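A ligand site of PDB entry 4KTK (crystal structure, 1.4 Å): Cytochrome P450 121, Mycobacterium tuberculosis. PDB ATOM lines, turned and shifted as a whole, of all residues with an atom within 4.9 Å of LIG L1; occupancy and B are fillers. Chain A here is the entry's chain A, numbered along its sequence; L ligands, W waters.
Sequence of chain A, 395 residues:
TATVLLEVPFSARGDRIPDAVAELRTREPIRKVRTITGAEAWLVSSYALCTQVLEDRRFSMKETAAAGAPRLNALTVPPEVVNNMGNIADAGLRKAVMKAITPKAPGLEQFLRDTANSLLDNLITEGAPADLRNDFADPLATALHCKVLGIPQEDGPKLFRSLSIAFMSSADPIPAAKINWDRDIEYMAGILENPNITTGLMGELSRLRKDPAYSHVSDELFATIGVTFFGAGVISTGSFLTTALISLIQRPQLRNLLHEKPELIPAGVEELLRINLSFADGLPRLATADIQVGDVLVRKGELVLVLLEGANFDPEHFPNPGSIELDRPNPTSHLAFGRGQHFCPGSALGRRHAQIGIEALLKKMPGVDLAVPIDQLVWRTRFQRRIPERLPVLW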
ATOM      1  N   LEU A  54     -16.375  -8.544  14.979  1.00  0.00           N
ATOM      2  CA  LEU A  54     -15.372  -8.773  15.981  1.00  0.00           C
ATOM      3  C   LEU A  54     -15.588  -8.130  17.432  1.00  0.00           C
ATOM      4  O   LEU A  54     -15.137  -8.621  18.402  1.00  0.00           O
ATOM      5  CB  LEU A  54     -13.975  -8.402  15.474  1.00  0.00           C
ATOM      6  CG  LEU A  54     -13.415  -9.237  14.335  1.00  0.00           C
ATOM      7  CD1 LEU A  54     -12.083  -8.722  13.922  1.00  0.00           C
ATOM      8  CD2 LEU A  54     -13.340 -10.675  14.668  1.00  0.00           C
ATOM      9  N   MET A  61     -16.300 -17.079  19.419  1.00  0.00           N
ATOM     10  CA  MET A  61     -15.209 -17.994  19.022  1.00  0.00           C
ATOM     11  C   MET A  61     -15.478 -19.324  19.624  1.00  0.00           C
ATOM     12  O   MET A  61     -15.382 -20.380  18.949  1.00  0.00           O
ATOM     13  CB  MET A  61     -13.790 -17.423  19.453  1.00  0.00           C
ATOM     14  CG  MET A  61     -12.668 -18.461  19.363  1.00  0.00           C
ATOM     15  SD  MET A  61     -11.139 -17.798  20.031  1.00  0.00           S
ATOM     16  CE  MET A  61     -10.763 -16.593  18.819  1.00  0.00           C
ATOM     17  N   ASN A  84      -9.303 -21.157  24.710  1.00  0.00           N
ATOM     18  CA  ASN A  84      -8.006 -21.151  25.477  1.00  0.00           C
ATOM     19  C   ASN A  84      -7.906 -19.896  26.243  1.00  0.00           C
ATOM     20  O   ASN A  84      -7.672 -19.915  27.495  1.00  0.00           O
ATOM     21  CB  ASN A  84      -6.847 -21.387  24.498  1.00  0.00           C
ATOM     22  CG  ASN A  84      -5.495 -21.624  25.178  1.00  0.00           C
ATOM     23  OD1 ASN A  84      -5.405 -22.334  26.209  1.00  0.00           O
ATOM     24  ND2 ASN A  84      -4.482 -21.061  24.570  1.00  0.00           N
ATOM     25  N   MET A  85      -8.150 -18.746  25.672  1.00  0.00           N
ATOM     26  CA  MET A  85      -8.050 -17.446  26.468  1.00  0.00           C
ATOM     27  C   MET A  85      -9.101 -17.310  27.542  1.00  0.00           C
ATOM     28  O   MET A  85      -8.852 -16.810  28.649  1.00  0.00           O
ATOM     29  CB  MET A  85      -7.990 -16.241  25.548  1.00  0.00           C
ATOM     30  CG  MET A  85      -6.544 -16.026  25.023  1.00  0.00           C
ATOM     31  SD  MET A  85      -5.075 -15.721  26.048  1.00  0.00           S
ATOM     32  CE  MET A  85      -5.702 -14.858  27.483  1.00  0.00           C
ATOM     33  N   ILE A 101       4.985 -12.539  28.213  1.00  0.00           N
ATOM     34  CA  ILE A 101       5.195 -12.570  26.758  1.00  0.00           C
ATOM     35  C   ILE A 101       5.366 -11.167  26.237  1.00  0.00           C
ATOM     36  O   ILE A 101       5.309 -10.910  25.008  1.00  0.00           O
ATOM     37  CB  ILE A 101       4.030 -13.314  26.025  1.00  0.00           C
ATOM     38  CG1 ILE A 101       2.719 -12.608  26.143  1.00  0.00           C
ATOM     39  CG2 ILE A 101       3.872 -14.720  26.609  1.00  0.00           C
ATOM     40  CD1 ILE A 101       1.507 -13.191  25.404  1.00  0.00           C
ATOM     41  N   HIS A 145      10.667 -17.827  20.910  1.00  0.00           N
ATOM     42  CA  HIS A 145       9.702 -18.467  21.760  1.00  0.00           C
ATOM     43  C   HIS A 145      10.231 -19.419  22.796  1.00  0.00           C
ATOM     44  O   HIS A 145       9.642 -19.524  23.894  1.00  0.00           O
ATOM     45  CB  HIS A 145       8.565 -19.041  20.911  1.00  0.00           C
ATOM     46  CG  HIS A 145       7.680 -17.972  20.341  1.00  0.00           C
ATOM     47  ND1 HIS A 145       8.014 -17.220  19.248  1.00  0.00           N
ATOM     48  CD2 HIS A 145       6.526 -17.431  20.814  1.00  0.00           C
ATOM     49  CE1 HIS A 145       7.126 -16.268  19.067  1.00  0.00           C
ATOM     50  NE2 HIS A 145       6.172 -16.367  19.982  1.00  0.00           N
ATOM     51  N   PHE A 229       0.840 -21.325  23.246  1.00  0.00           N
ATOM     52  CA  PHE A 229       1.538 -20.037  23.058  1.00  0.00           C
ATOM     53  C   PHE A 229       2.824 -20.268  22.255  1.00  0.00           C
ATOM     54  O   PHE A 229       3.074 -19.409  21.377  1.00  0.00           O
ATOM     55  CB  PHE A 229       1.798 -19.323  24.460  1.00  0.00           C
ATOM     56  CG  PHE A 229       0.612 -18.535  24.919  1.00  0.00           C
ATOM     57  CD1 PHE A 229      -0.649 -19.153  25.187  1.00  0.00           C
ATOM     58  CD2 PHE A 229       0.599 -17.143  24.798  1.00  0.00           C
ATOM     59  CE1 PHE A 229      -1.750 -18.386  25.546  1.00  0.00           C
ATOM     60  CE2 PHE A 229      -0.514 -16.381  25.171  1.00  0.00           C
ATOM     61  CZ  PHE A 229      -1.700 -17.006  25.515  1.00  0.00           C
ATOM     62  N   ALA A 232       1.192 -20.949  18.471  1.00  0.00           N
ATOM     63  CA  ALA A 232       0.631 -19.737  17.888  1.00  0.00           C
ATOM     64  C   ALA A 232       1.607 -18.605  17.630  1.00  0.00           C
ATOM     65  O   ALA A 232       1.645 -18.008  16.595  1.00  0.00           O
ATOM     66  CB  ALA A 232      -0.544 -19.180  18.690  1.00  0.00           C
ATOM     67  N   GLY A 233       2.472 -18.395  18.614  1.00  0.00           N
ATOM     68  CA  GLY A 233       3.509 -17.416  18.444  1.00  0.00           C
ATOM     69  C   GLY A 233       4.479 -17.709  17.338  1.00  0.00           C
ATOM     70  O   GLY A 233       4.819 -16.810  16.537  1.00  0.00           O
ATOM     71  N   SER A 236       2.820 -17.591  13.863  1.00  0.00           N
ATOM     72  CA  SER A 236       2.370 -16.271  13.483  1.00  0.00           C
ATOM     73  C   SER A 236       3.488 -15.272  13.184  1.00  0.00           C
ATOM     74  O   SER A 236       3.481 -14.606  12.166  1.00  0.00           O
ATOM     75  CB  SER A 236       1.433 -15.681  14.539  1.00  0.00           C
ATOM     76  OG  SER A 236       0.253 -16.524  14.763  1.00  0.00           O
ATOM     77  N   THR A 237       4.501 -15.315  14.047  1.00  0.00           N
ATOM     78  CA  THR A 237       5.678 -14.453  13.869  1.00  0.00           C
ATOM     79  C   THR A 237       6.513 -14.910  12.709  1.00  0.00           C
ATOM     80  O   THR A 237       6.982 -14.070  11.858  1.00  0.00           O
ATOM     81  CB  THR A 237       6.510 -14.342  15.156  1.00  0.00           C
ATOM     82  OG1 THR A 237       7.034 -15.570  15.565  1.00  0.00           O
ATOM     83  CG2 THR A 237       5.718 -13.607  16.266  1.00  0.00           C
ATOM     84  N   PHE A 240       4.443 -14.146   9.475  1.00  0.00           N
ATOM     85  CA  PHE A 240       4.367 -12.716   9.220  1.00  0.00           C
ATOM     86  C   PHE A 240       5.709 -12.122   8.792  1.00  0.00           C
ATOM     87  O   PHE A 240       5.791 -11.464   7.790  1.00  0.00           O
ATOM     88  CB  PHE A 240       3.856 -11.901  10.433  1.00  0.00           C
ATOM     89  CG  PHE A 240       4.001 -10.411  10.211  1.00  0.00           C
ATOM     90  CD1 PHE A 240       3.301  -9.792   9.190  1.00  0.00           C
ATOM     91  CD2 PHE A 240       4.934  -9.688  10.890  1.00  0.00           C
ATOM     92  CE1 PHE A 240       3.482  -8.465   8.866  1.00  0.00           C
ATOM     93  CE2 PHE A 240       5.115  -8.371  10.577  1.00  0.00           C
ATOM     94  CZ  PHE A 240       4.433  -7.768   9.579  1.00  0.00           C
ATOM     95  N   LEU A 273       2.252  -4.951   8.528  1.00  0.00           N
ATOM     96  CA  LEU A 273       1.144  -5.642   9.198  1.00  0.00           C
ATOM     97  C   LEU A 273      -0.149  -5.381   8.535  1.00  0.00           C
ATOM     98  O   LEU A 273      -0.970  -6.300   8.243  1.00  0.00           O
ATOM     99  CB  LEU A 273       1.055  -5.255  10.727  1.00  0.00           C
ATOM    100  CG  LEU A 273       2.120  -5.882  11.548  1.00  0.00           C
ATOM    101  CD1 LEU A 273       2.336  -5.157  12.850  1.00  0.00           C
ATOM    102  CD2 LEU A 273       1.729  -7.339  11.862  1.00  0.00           C
ATOM    103  N   PHE A 279      -2.793 -14.590   7.217  1.00  0.00           N
ATOM    104  CA  PHE A 279      -3.966 -15.421   7.574  1.00  0.00           C
ATOM    105  C   PHE A 279      -4.652 -15.874   6.334  1.00  0.00           C
ATOM    106  O   PHE A 279      -5.155 -15.142   5.536  1.00  0.00           O
ATOM    107  CB  PHE A 279      -4.934 -14.654   8.562  1.00  0.00           C
ATOM    108  CG  PHE A 279      -4.532 -14.708  10.010  1.00  0.00           C
ATOM    109  CD1 PHE A 279      -3.337 -14.199  10.379  1.00  0.00           C
ATOM    110  CD2 PHE A 279      -5.335 -15.344  10.930  1.00  0.00           C
ATOM    111  CE1 PHE A 279      -2.913 -14.319  11.739  1.00  0.00           C
ATOM    112  CE2 PHE A 279      -4.903 -15.456  12.258  1.00  0.00           C
ATOM    113  CZ  PHE A 279      -3.745 -14.940  12.627  1.00  0.00           C
ATOM    114  N   LEU A 283     -11.373 -15.112   9.979  1.00  0.00           N
ATOM    115  CA  LEU A 283     -11.484 -15.490  11.375  1.00  0.00           C
ATOM    116  C   LEU A 283     -12.900 -16.008  11.647  1.00  0.00           C
ATOM    117  O   LEU A 283     -13.874 -15.303  11.327  1.00  0.00           O
ATOM    118  CB  LEU A 283     -11.276 -14.303  12.397  1.00  0.00           C
ATOM    119  CG  LEU A 283      -9.933 -13.580  12.237  1.00  0.00           C
ATOM    120  CD1 LEU A 283      -9.822 -12.499  13.246  1.00  0.00           C
ATOM    121  CD2 LEU A 283      -8.746 -14.584  12.363  1.00  0.00           C
ATOM    122  N   ARG A 285     -16.376 -17.196  13.497  1.00  0.00           N
ATOM    123  CA  ARG A 285     -17.253 -16.922  14.646  1.00  0.00           C
ATOM    124  C   ARG A 285     -18.607 -17.583  14.425  1.00  0.00           C
ATOM    125  O   ARG A 285     -19.014 -17.639  13.259  1.00  0.00           O
ATOM    126  CB  ARG A 285     -17.518 -15.397  14.772  1.00  0.00           C
ATOM    127  CG  ARG A 285     -16.290 -14.545  15.122  1.00  0.00           C
ATOM    128  CD  ARG A 285     -15.783 -14.854  16.480  1.00  0.00           C
ATOM    129  NE  ARG A 285     -14.722 -13.903  16.891  1.00  0.00           N
ATOM    130  CZ  ARG A 285     -13.436 -14.039  16.696  1.00  0.00           C
ATOM    131  NH1 ARG A 285     -12.930 -15.083  16.085  1.00  0.00           N
ATOM    132  NH2 ARG A 285     -12.590 -13.119  17.187  1.00  0.00           N
ATOM    133  N   LEU A 308      -9.679 -10.584   7.192  1.00  0.00           N
ATOM    134  CA  LEU A 308      -8.781  -9.500   7.693  1.00  0.00           C
ATOM    135  C   LEU A 308      -8.392  -8.674   6.510  1.00  0.00           C
ATOM    136  O   LEU A 308      -8.293  -7.382   6.664  1.00  0.00           O
ATOM    137  CB  LEU A 308      -7.591 -10.070   8.464  1.00  0.00           C
ATOM    138  CG  LEU A 308      -7.992 -10.805   9.767  1.00  0.00           C
ATOM    139  CD1 LEU A 308      -6.719 -11.234  10.403  1.00  0.00           C
ATOM    140  CD2 LEU A 308      -8.947 -10.038  10.630  1.00  0.00           C
ATOM    141  N   LEU A 335      -6.610  -4.467  11.313  1.00  0.00           N
ATOM    142  CA  LEU A 335      -7.098  -5.705  12.038  1.00  0.00           C
ATOM    143  C   LEU A 335      -6.109  -6.822  11.942  1.00  0.00           C
ATOM    144  O   LEU A 335      -6.487  -8.017  12.176  1.00  0.00           O
ATOM    145  CB  LEU A 335      -8.449  -6.128  11.489  1.00  0.00           C
ATOM    146  CG  LEU A 335      -9.572  -5.048  11.417  1.00  0.00           C
ATOM    147  CD1 LEU A 335     -10.905  -5.709  11.215  1.00  0.00           C
ATOM    148  CD2 LEU A 335      -9.670  -4.259  12.669  1.00  0.00           C
ATOM    149  N   ALA A 336      -4.840  -6.595  11.721  1.00  0.00           N
ATOM    150  CA  ALA A 336      -3.868  -7.700  11.656  1.00  0.00           C
ATOM    151  C   ALA A 336      -3.810  -8.491  12.902  1.00  0.00           C
ATOM    152  O   ALA A 336      -3.446  -9.696  12.790  1.00  0.00           O
ATOM    153  CB  ALA A 336      -2.474  -7.189  11.323  1.00  0.00           C
ATOM    154  N   PHE A 337      -4.052  -7.970  14.094  1.00  0.00           N
ATOM    155  CA  PHE A 337      -4.045  -8.685  15.353  1.00  0.00           C
ATOM    156  C   PHE A 337      -5.478  -8.950  15.843  1.00  0.00           C
ATOM    157  O   PHE A 337      -5.692  -9.281  17.021  1.00  0.00           O
ATOM    158  CB  PHE A 337      -3.267  -7.851  16.406  1.00  0.00           C
ATOM    159  CG  PHE A 337      -1.816  -7.739  16.064  1.00  0.00           C
ATOM    160  CD1 PHE A 337      -0.996  -8.863  16.123  1.00  0.00           C
ATOM    161  CD2 PHE A 337      -1.206  -6.477  15.915  1.00  0.00           C
ATOM    162  CE1 PHE A 337       0.312  -8.748  15.838  1.00  0.00           C
ATOM    163  CE2 PHE A 337       0.122  -6.418  15.598  1.00  0.00           C
ATOM    164  CZ  PHE A 337       0.885  -7.500  15.679  1.00  0.00           C
ATOM    165  N   GLY A 338      -6.445  -8.801  14.977  1.00  0.00           N
ATOM    166  CA  GLY A 338      -7.875  -8.933  15.329  1.00  0.00           C
ATOM    167  C   GLY A 338      -8.376  -7.647  16.023  1.00  0.00           C
ATOM    168  O   GLY A 338      -7.824  -6.533  15.849  1.00  0.00           O
ATOM    169  N   GLN A 341     -12.736  -8.851  21.982  1.00  0.00           N
ATOM    170  CA  GLN A 341     -12.379  -9.785  23.112  1.00  0.00           C
ATOM    171  C   GLN A 341     -11.132 -10.654  22.824  1.00  0.00           C
ATOM    172  O   GLN A 341     -10.403 -11.019  23.748  1.00  0.00           O
ATOM    173  CB  GLN A 341     -13.603 -10.704  23.270  1.00  0.00           C
ATOM    174  CG  GLN A 341     -13.472 -11.735  24.363  1.00  0.00           C
ATOM    175  CD  GLN A 341     -13.663 -11.221  25.746  1.00  0.00           C
ATOM    176  OE1 GLN A 341     -13.424 -11.995  26.701  1.00  0.00           O
ATOM    177  NE2 GLN A 341     -14.132  -9.959  25.913  1.00  0.00           N
ATOM    178  N   HIS A 342     -10.966 -11.074  21.565  1.00  0.00           N
ATOM    179  CA  HIS A 342      -9.927 -11.959  21.218  1.00  0.00           C
ATOM    180  C   HIS A 342      -8.742 -11.360  20.537  1.00  0.00           C
ATOM    181  O   HIS A 342      -7.870 -12.047  19.921  1.00  0.00           O
ATOM    182  CB  HIS A 342     -10.527 -13.087  20.337  1.00  0.00           C
ATOM    183  CG  HIS A 342     -11.526 -13.903  21.079  1.00  0.00           C
ATOM    184  ND1 HIS A 342     -11.169 -14.688  22.170  1.00  0.00           N
ATOM    185  CD2 HIS A 342     -12.882 -13.958  20.992  1.00  0.00           C
ATOM    186  CE1 HIS A 342     -12.254 -15.273  22.667  1.00  0.00           C
ATOM    187  NE2 HIS A 342     -13.300 -14.841  21.992  1.00  0.00           N
ATOM    188  N   PHE A 343      -8.545 -10.040  20.729  1.00  0.00           N
ATOM    189  CA  PHE A 343      -7.358  -9.349  20.207  1.00  0.00           C
ATOM    190  C   PHE A 343      -6.093 -10.078  20.614  1.00  0.00           C
ATOM    191  O   PHE A 343      -5.944 -10.535  21.763  1.00  0.00           O
ATOM    192  CB  PHE A 343      -7.331  -7.895  20.756  1.00  0.00           C
ATOM    193  CG  PHE A 343      -6.185  -7.040  20.222  1.00  0.00           C
ATOM    194  CD1 PHE A 343      -6.318  -6.427  19.050  1.00  0.00           C
ATOM    195  CD2 PHE A 343      -4.988  -6.926  20.865  1.00  0.00           C
ATOM    196  CE1 PHE A 343      -5.329  -5.591  18.526  1.00  0.00           C
ATOM    197  CE2 PHE A 343      -3.957  -6.170  20.305  1.00  0.00           C
ATOM    198  CZ  PHE A 343      -4.114  -5.554  19.127  1.00  0.00           C
ATOM    199  N   CYS A 344      -5.150 -10.212  19.709  1.00  0.00           N
ATOM    200  CA  CYS A 344      -3.938 -10.994  19.928  1.00  0.00           C
ATOM    201  C   CYS A 344      -3.235 -10.587  21.260  1.00  0.00           C
ATOM    202  O   CYS A 344      -2.761  -9.438  21.415  1.00  0.00           O
ATOM    203  CB  CYS A 344      -2.979 -10.809  18.777  1.00  0.00           C
ATOM    204  SG  CYS A 344      -1.455 -11.735  18.973  1.00  0.00           S
ATOM    205  N   PRO A 345      -2.985 -11.590  22.124  1.00  0.00           N
ATOM    206  CA  PRO A 345      -2.299 -11.286  23.402  1.00  0.00           C
ATOM    207  C   PRO A 345      -0.772 -11.096  23.153  1.00  0.00           C
ATOM    208  O   PRO A 345      -0.038 -10.554  24.005  1.00  0.00           O
ATOM    209  CB  PRO A 345      -2.591 -12.547  24.256  1.00  0.00           C
ATOM    210  CG  PRO A 345      -2.696 -13.659  23.295  1.00  0.00           C
ATOM    211  CD  PRO A 345      -3.464 -13.025  22.169  1.00  0.00           C
ATOM    212  N   GLY A 346      -0.265 -11.525  22.028  1.00  0.00           N
ATOM    213  CA  GLY A 346       1.196 -11.448  21.654  1.00  0.00           C
ATOM    214  C   GLY A 346       1.565 -10.307  20.669  1.00  0.00           C
ATOM    215  O   GLY A 346       2.677 -10.254  20.170  1.00  0.00           O
ATOM    216  N   LEU A 349       4.960  -8.508  21.203  1.00  0.00           N
ATOM    217  CA  LEU A 349       6.019  -9.413  20.866  1.00  0.00           C
ATOM    218  C   LEU A 349       6.170  -9.583  19.376  1.00  0.00           C
ATOM    219  O   LEU A 349       7.258  -9.631  18.844  1.00  0.00           O
ATOM    220  CB  LEU A 349       5.846 -10.725  21.583  1.00  0.00           C
ATOM    221  CG  LEU A 349       6.980 -11.682  21.573  1.00  0.00           C
ATOM    222  CD1 LEU A 349       8.215 -11.093  22.306  1.00  0.00           C
ATOM    223  CD2 LEU A 349       6.585 -12.972  22.180  1.00  0.00           C
ATOM    224  N   GLY A 350       5.027  -9.716  18.704  1.00  0.00           N
ATOM    225  CA  GLY A 350       5.055  -9.923  17.273  1.00  0.00           C
ATOM    226  C   GLY A 350       5.632  -8.708  16.533  1.00  0.00           C
ATOM    227  O   GLY A 350       6.487  -8.829  15.655  1.00  0.00           O
HETATM  228  C1  LIG L   1      -4.947 -14.396  18.452  1.00  0.00           C
HETATM  229  C2  LIG L   1      -2.519 -12.408  14.785  1.00  0.00           C
HETATM  230  C3  LIG L   1       1.641 -13.180  17.258  1.00  0.00           C
HETATM  231  C4  LIG L   1      -0.785 -15.785  20.487  1.00  0.00           C
HETATM  232  C5  LIG L   1      -4.684 -13.670  17.302  1.00  0.00           C
HETATM  233  C6  LIG L   1      -5.620 -13.156  16.342  1.00  0.00           C
HETATM  234  C7  LIG L   1      -4.987 -12.647  15.299  1.00  0.00           C
HETATM  235  C8  LIG L   1      -3.546 -12.840  15.567  1.00  0.00           C
HETATM  236  C9  LIG L   1      -5.452 -12.025  14.068  1.00  0.00           C
HETATM  237  C10 LIG L   1      -7.124 -13.122  16.600  1.00  0.00           C
HETATM  238  C11 LIG L   1      -7.852 -14.365  16.222  1.00  0.00           C
HETATM  239  C12 LIG L   1      -9.310 -14.301  16.381  1.00  0.00           C
HETATM  240  O1  LIG L   1      -9.879 -13.299  16.882  1.00  0.00           O
HETATM  241  O2  LIG L   1     -10.031 -15.260  15.953  1.00  0.00           O
HETATM  242  C13 LIG L   1      -1.125 -12.464  15.093  1.00  0.00           C
HETATM  243  C14 LIG L   1      -0.084 -11.945  14.301  1.00  0.00           C
HETATM  244  C15 LIG L   1       1.127 -12.151  14.970  1.00  0.00           C
HETATM  245  C16 LIG L   1       0.781 -12.815  16.238  1.00  0.00           C
HETATM  246  C17 LIG L   1      -0.228 -11.300  12.997  1.00  0.00           C
HETATM  247  C18 LIG L   1       2.492 -11.742  14.642  1.00  0.00           C
HETATM  248  C19 LIG L   1       2.787 -10.831  13.807  1.00  0.00           C
HETATM  249  C20 LIG L   1       1.371 -13.876  18.427  1.00  0.00           C
HETATM  250  C21 LIG L   1       2.326 -14.261  19.425  1.00  0.00           C
HETATM  251  C22 LIG L   1       1.607 -15.017  20.261  1.00  0.00           C
HETATM  252  C23 LIG L   1       0.245 -15.131  19.846  1.00  0.00           C
HETATM  253  C24 LIG L   1       3.746 -13.761  19.422  1.00  0.00           C
HETATM  254  C25 LIG L   1       2.127 -15.643  21.494  1.00  0.00           C
HETATM  255  C26 LIG L   1       3.407 -15.791  21.917  1.00  0.00           C
HETATM  256  C27 LIG L   1      -2.116 -15.735  20.161  1.00  0.00           C
HETATM  257  C28 LIG L   1      -3.217 -16.397  20.875  1.00  0.00           C
HETATM  258  C29 LIG L   1      -4.399 -15.938  20.327  1.00  0.00           C
HETATM  259  C30 LIG L   1      -4.041 -15.066  19.245  1.00  0.00           C
HETATM  260  C31 LIG L   1      -3.009 -17.291  22.058  1.00  0.00           C
HETATM  261  C32 LIG L   1      -5.795 -16.355  20.736  1.00  0.00           C
HETATM  262  C33 LIG L   1      -6.475 -15.305  21.571  1.00  0.00           C
HETATM  263  C34 LIG L   1      -7.962 -15.567  21.962  1.00  0.00           C
HETATM  264  O3  LIG L   1      -8.493 -14.683  22.640  1.00  0.00           O
HETATM  265  O4  LIG L   1      -8.435 -16.638  21.714  1.00  0.00           O
HETATM  266  N1  LIG L   1      -3.423 -13.472  16.819  1.00  0.00           N
HETATM  267  N2  LIG L   1      -0.596 -12.939  16.243  1.00  0.00           N
HETATM  268  N3  LIG L   1       0.111 -14.310  18.699  1.00  0.00           N
HETATM  269  N4  LIG L   1      -2.670 -14.837  19.220  1.00  0.00           N
HETATM  270 FE1  LIG L   1      -1.659 -13.820  17.804  1.00  0.00          FE
HETATM  271  C1  LG2 L   2      -3.499 -21.952  18.960  1.00  0.00           C
HETATM  272  C2  LG2 L   2      -3.758 -21.105  20.018  1.00  0.00           C
HETATM  273  C3  LG2 L   2      -4.910 -21.183  20.706  1.00  0.00           C
HETATM  274  O1  LG2 L   2      -5.203 -20.308  21.705  1.00  0.00           O
HETATM  275  C4  LG2 L   2      -5.920 -22.016  20.274  1.00  0.00           C
HETATM  276  C5  LG2 L   2      -5.644 -22.803  19.117  1.00  0.00           C
HETATM  277  C6  LG2 L   2      -4.410 -22.814  18.477  1.00  0.00           C
HETATM  278  C7  LG2 L   2      -4.237 -23.555  17.320  1.00  0.00           C
HETATM  279  C8  LG2 L   2      -5.031 -23.394  16.141  1.00  0.00           C
HETATM  280  N1  LG2 L   2      -5.925 -22.394  15.824  1.00  0.00           N
HETATM  281  N2  LG2 L   2      -4.775 -24.326  15.199  1.00  0.00           N
HETATM  282  N3  LG2 L   2      -3.800 -25.080  15.760  1.00  0.00           N
HETATM  283  C9  LG2 L   2      -3.472 -24.629  17.038  1.00  0.00           C
HETATM  284  C10 LG2 L   2      -2.460 -25.334  17.718  1.00  0.00           C
HETATM  285  C11 LG2 L   2      -1.441 -24.663  18.517  1.00  0.00           C
HETATM  286  C12 LG2 L   2      -0.356 -25.366  19.013  1.00  0.00           C
HETATM  287  C13 LG2 L   2      -0.194 -26.716  18.718  1.00  0.00           C
HETATM  288  O2  LG2 L   2       0.882 -27.420  19.138  1.00  0.00           O
HETATM  289  C14 LG2 L   2      -1.198 -27.382  18.055  1.00  0.00           C
HETATM  290  C15 LG2 L   2      -2.175 -26.684  17.443  1.00  0.00           C
HETATM  291  O3  LG2 L   2      -3.078 -27.507  16.710  1.00  0.00           O
HETATM  292  O   HOH W   1      -9.871 -10.637  17.411  1.00  0.00           O
HETATM  293  O   HOH W   2      -7.699 -19.438  21.636  1.00  0.00           O
HETATM  294  O   HOH W   3     -10.234 -18.049  23.611  1.00  0.00           O
HETATM  295  O   HOH W   4      -9.186 -17.608  15.077  1.00  0.00           O
HETATM  296  O   HOH W   5      -6.962 -12.581  23.409  1.00  0.00           O
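The side-chain sulfur (SG) of Cys 344 binds an iron atom (FE1) of LIG L1.
An oxygen (O3) of LIG L1 lies within hydrogen-bond range of a ring nitrogen (ND1) of His 342 (2.7 Å).
The guanidinium group of Arg 285 is in salt-bridge range of an oxygen (O1) of LIG L1 (2.7 Å).
The side-chain amide nitrogen (ND2) of Asn 84 is in hydrogen-bond range of an oxygen (O1) of LG2 L2, 3.0 Å away.
O of Ala 232 lies within hydrogen-bond range of OG of Ser 236 (2.7 Å).
The backbone NH of Gly 346 sits close to the side-chain sulfur of Cys 344, 3.3 Å away.
N of Cys 344 sits at hydrogen-bond distance from O of Phe 337 (2.9 Å).
The side-chain sulfur (SD) of Met 61 is in hydrogen-bond range of a ring nitrogen (ND1) of His 342 (3.8 Å).
The side-chain hydroxyl of Thr 237 sits at hydrogen-bond distance from the backbone carbonyl oxygen of Gly 233.
An oxygen (O4) of LIG L1 lies close to the side-chain sulfur (SD) of Met 61, 3.4 Å away.
CB of Met 85 touches O3 of LIG L1, at 3.3 Å.
His 145 touches LIG L1 (NE2 to C26, 3.4 Å).
O of Phe 229 touches C26 of LIG L1, at 3.7 Å.
Ala 232 touches LIG L1.
CA of Gly 233 touches C21 of LIG L1 (3.5 Å).
CB of Ser 236 touches C16 of LIG L1, at 3.4 Å.
Thr 237 touches LIG L1.
Phe 240 touches LIG L1 (CB to C19, 3.7 Å).
CZ of Phe 279 touches C2 of LIG L1, at 3.5 Å.
Leu 283 touches LIG L1 (CD1 to C12, 3.7 Å).
Leu 308 touches LIG L1.
Ala 336 touches LIG L1 (O to C9, 3.3 Å).
C of Phe 337 touches C9 of LIG L1 (3.6 Å).
Gly 338 touches LIG L1.
Pro 345 touches LIG L1.
Gly 346 touches LIG L1.
Hydrophobic or aromatic side chains that line LIG L1: Met 61, Met 85, His 145, Phe 229, Ala 232, Phe 240, Phe 279, Leu 283, Leu 308, Phe 337, His 342 and Pro 345.
Water W5 lies within hydrogen-bond range of O3 of LIG L1 (2.7 Å) and O of Phe 343 (2.8 Å).
Water W2 bridges an oxygen (O1) of LG2 L2 (2.6 Å) and an oxygen (O4) of LIG L1 (2.9 Å).
Water W3 lies within hydrogen-bond range of an oxygen (O4) of LIG L1 (3.0 Å), the backbone NH (N) of Met 85 (3.0 Å), the backbone NH (N) of Asn 84 (3.4 Å) and the side-chain sulfur (SD) of Met 61 (3.7 Å).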
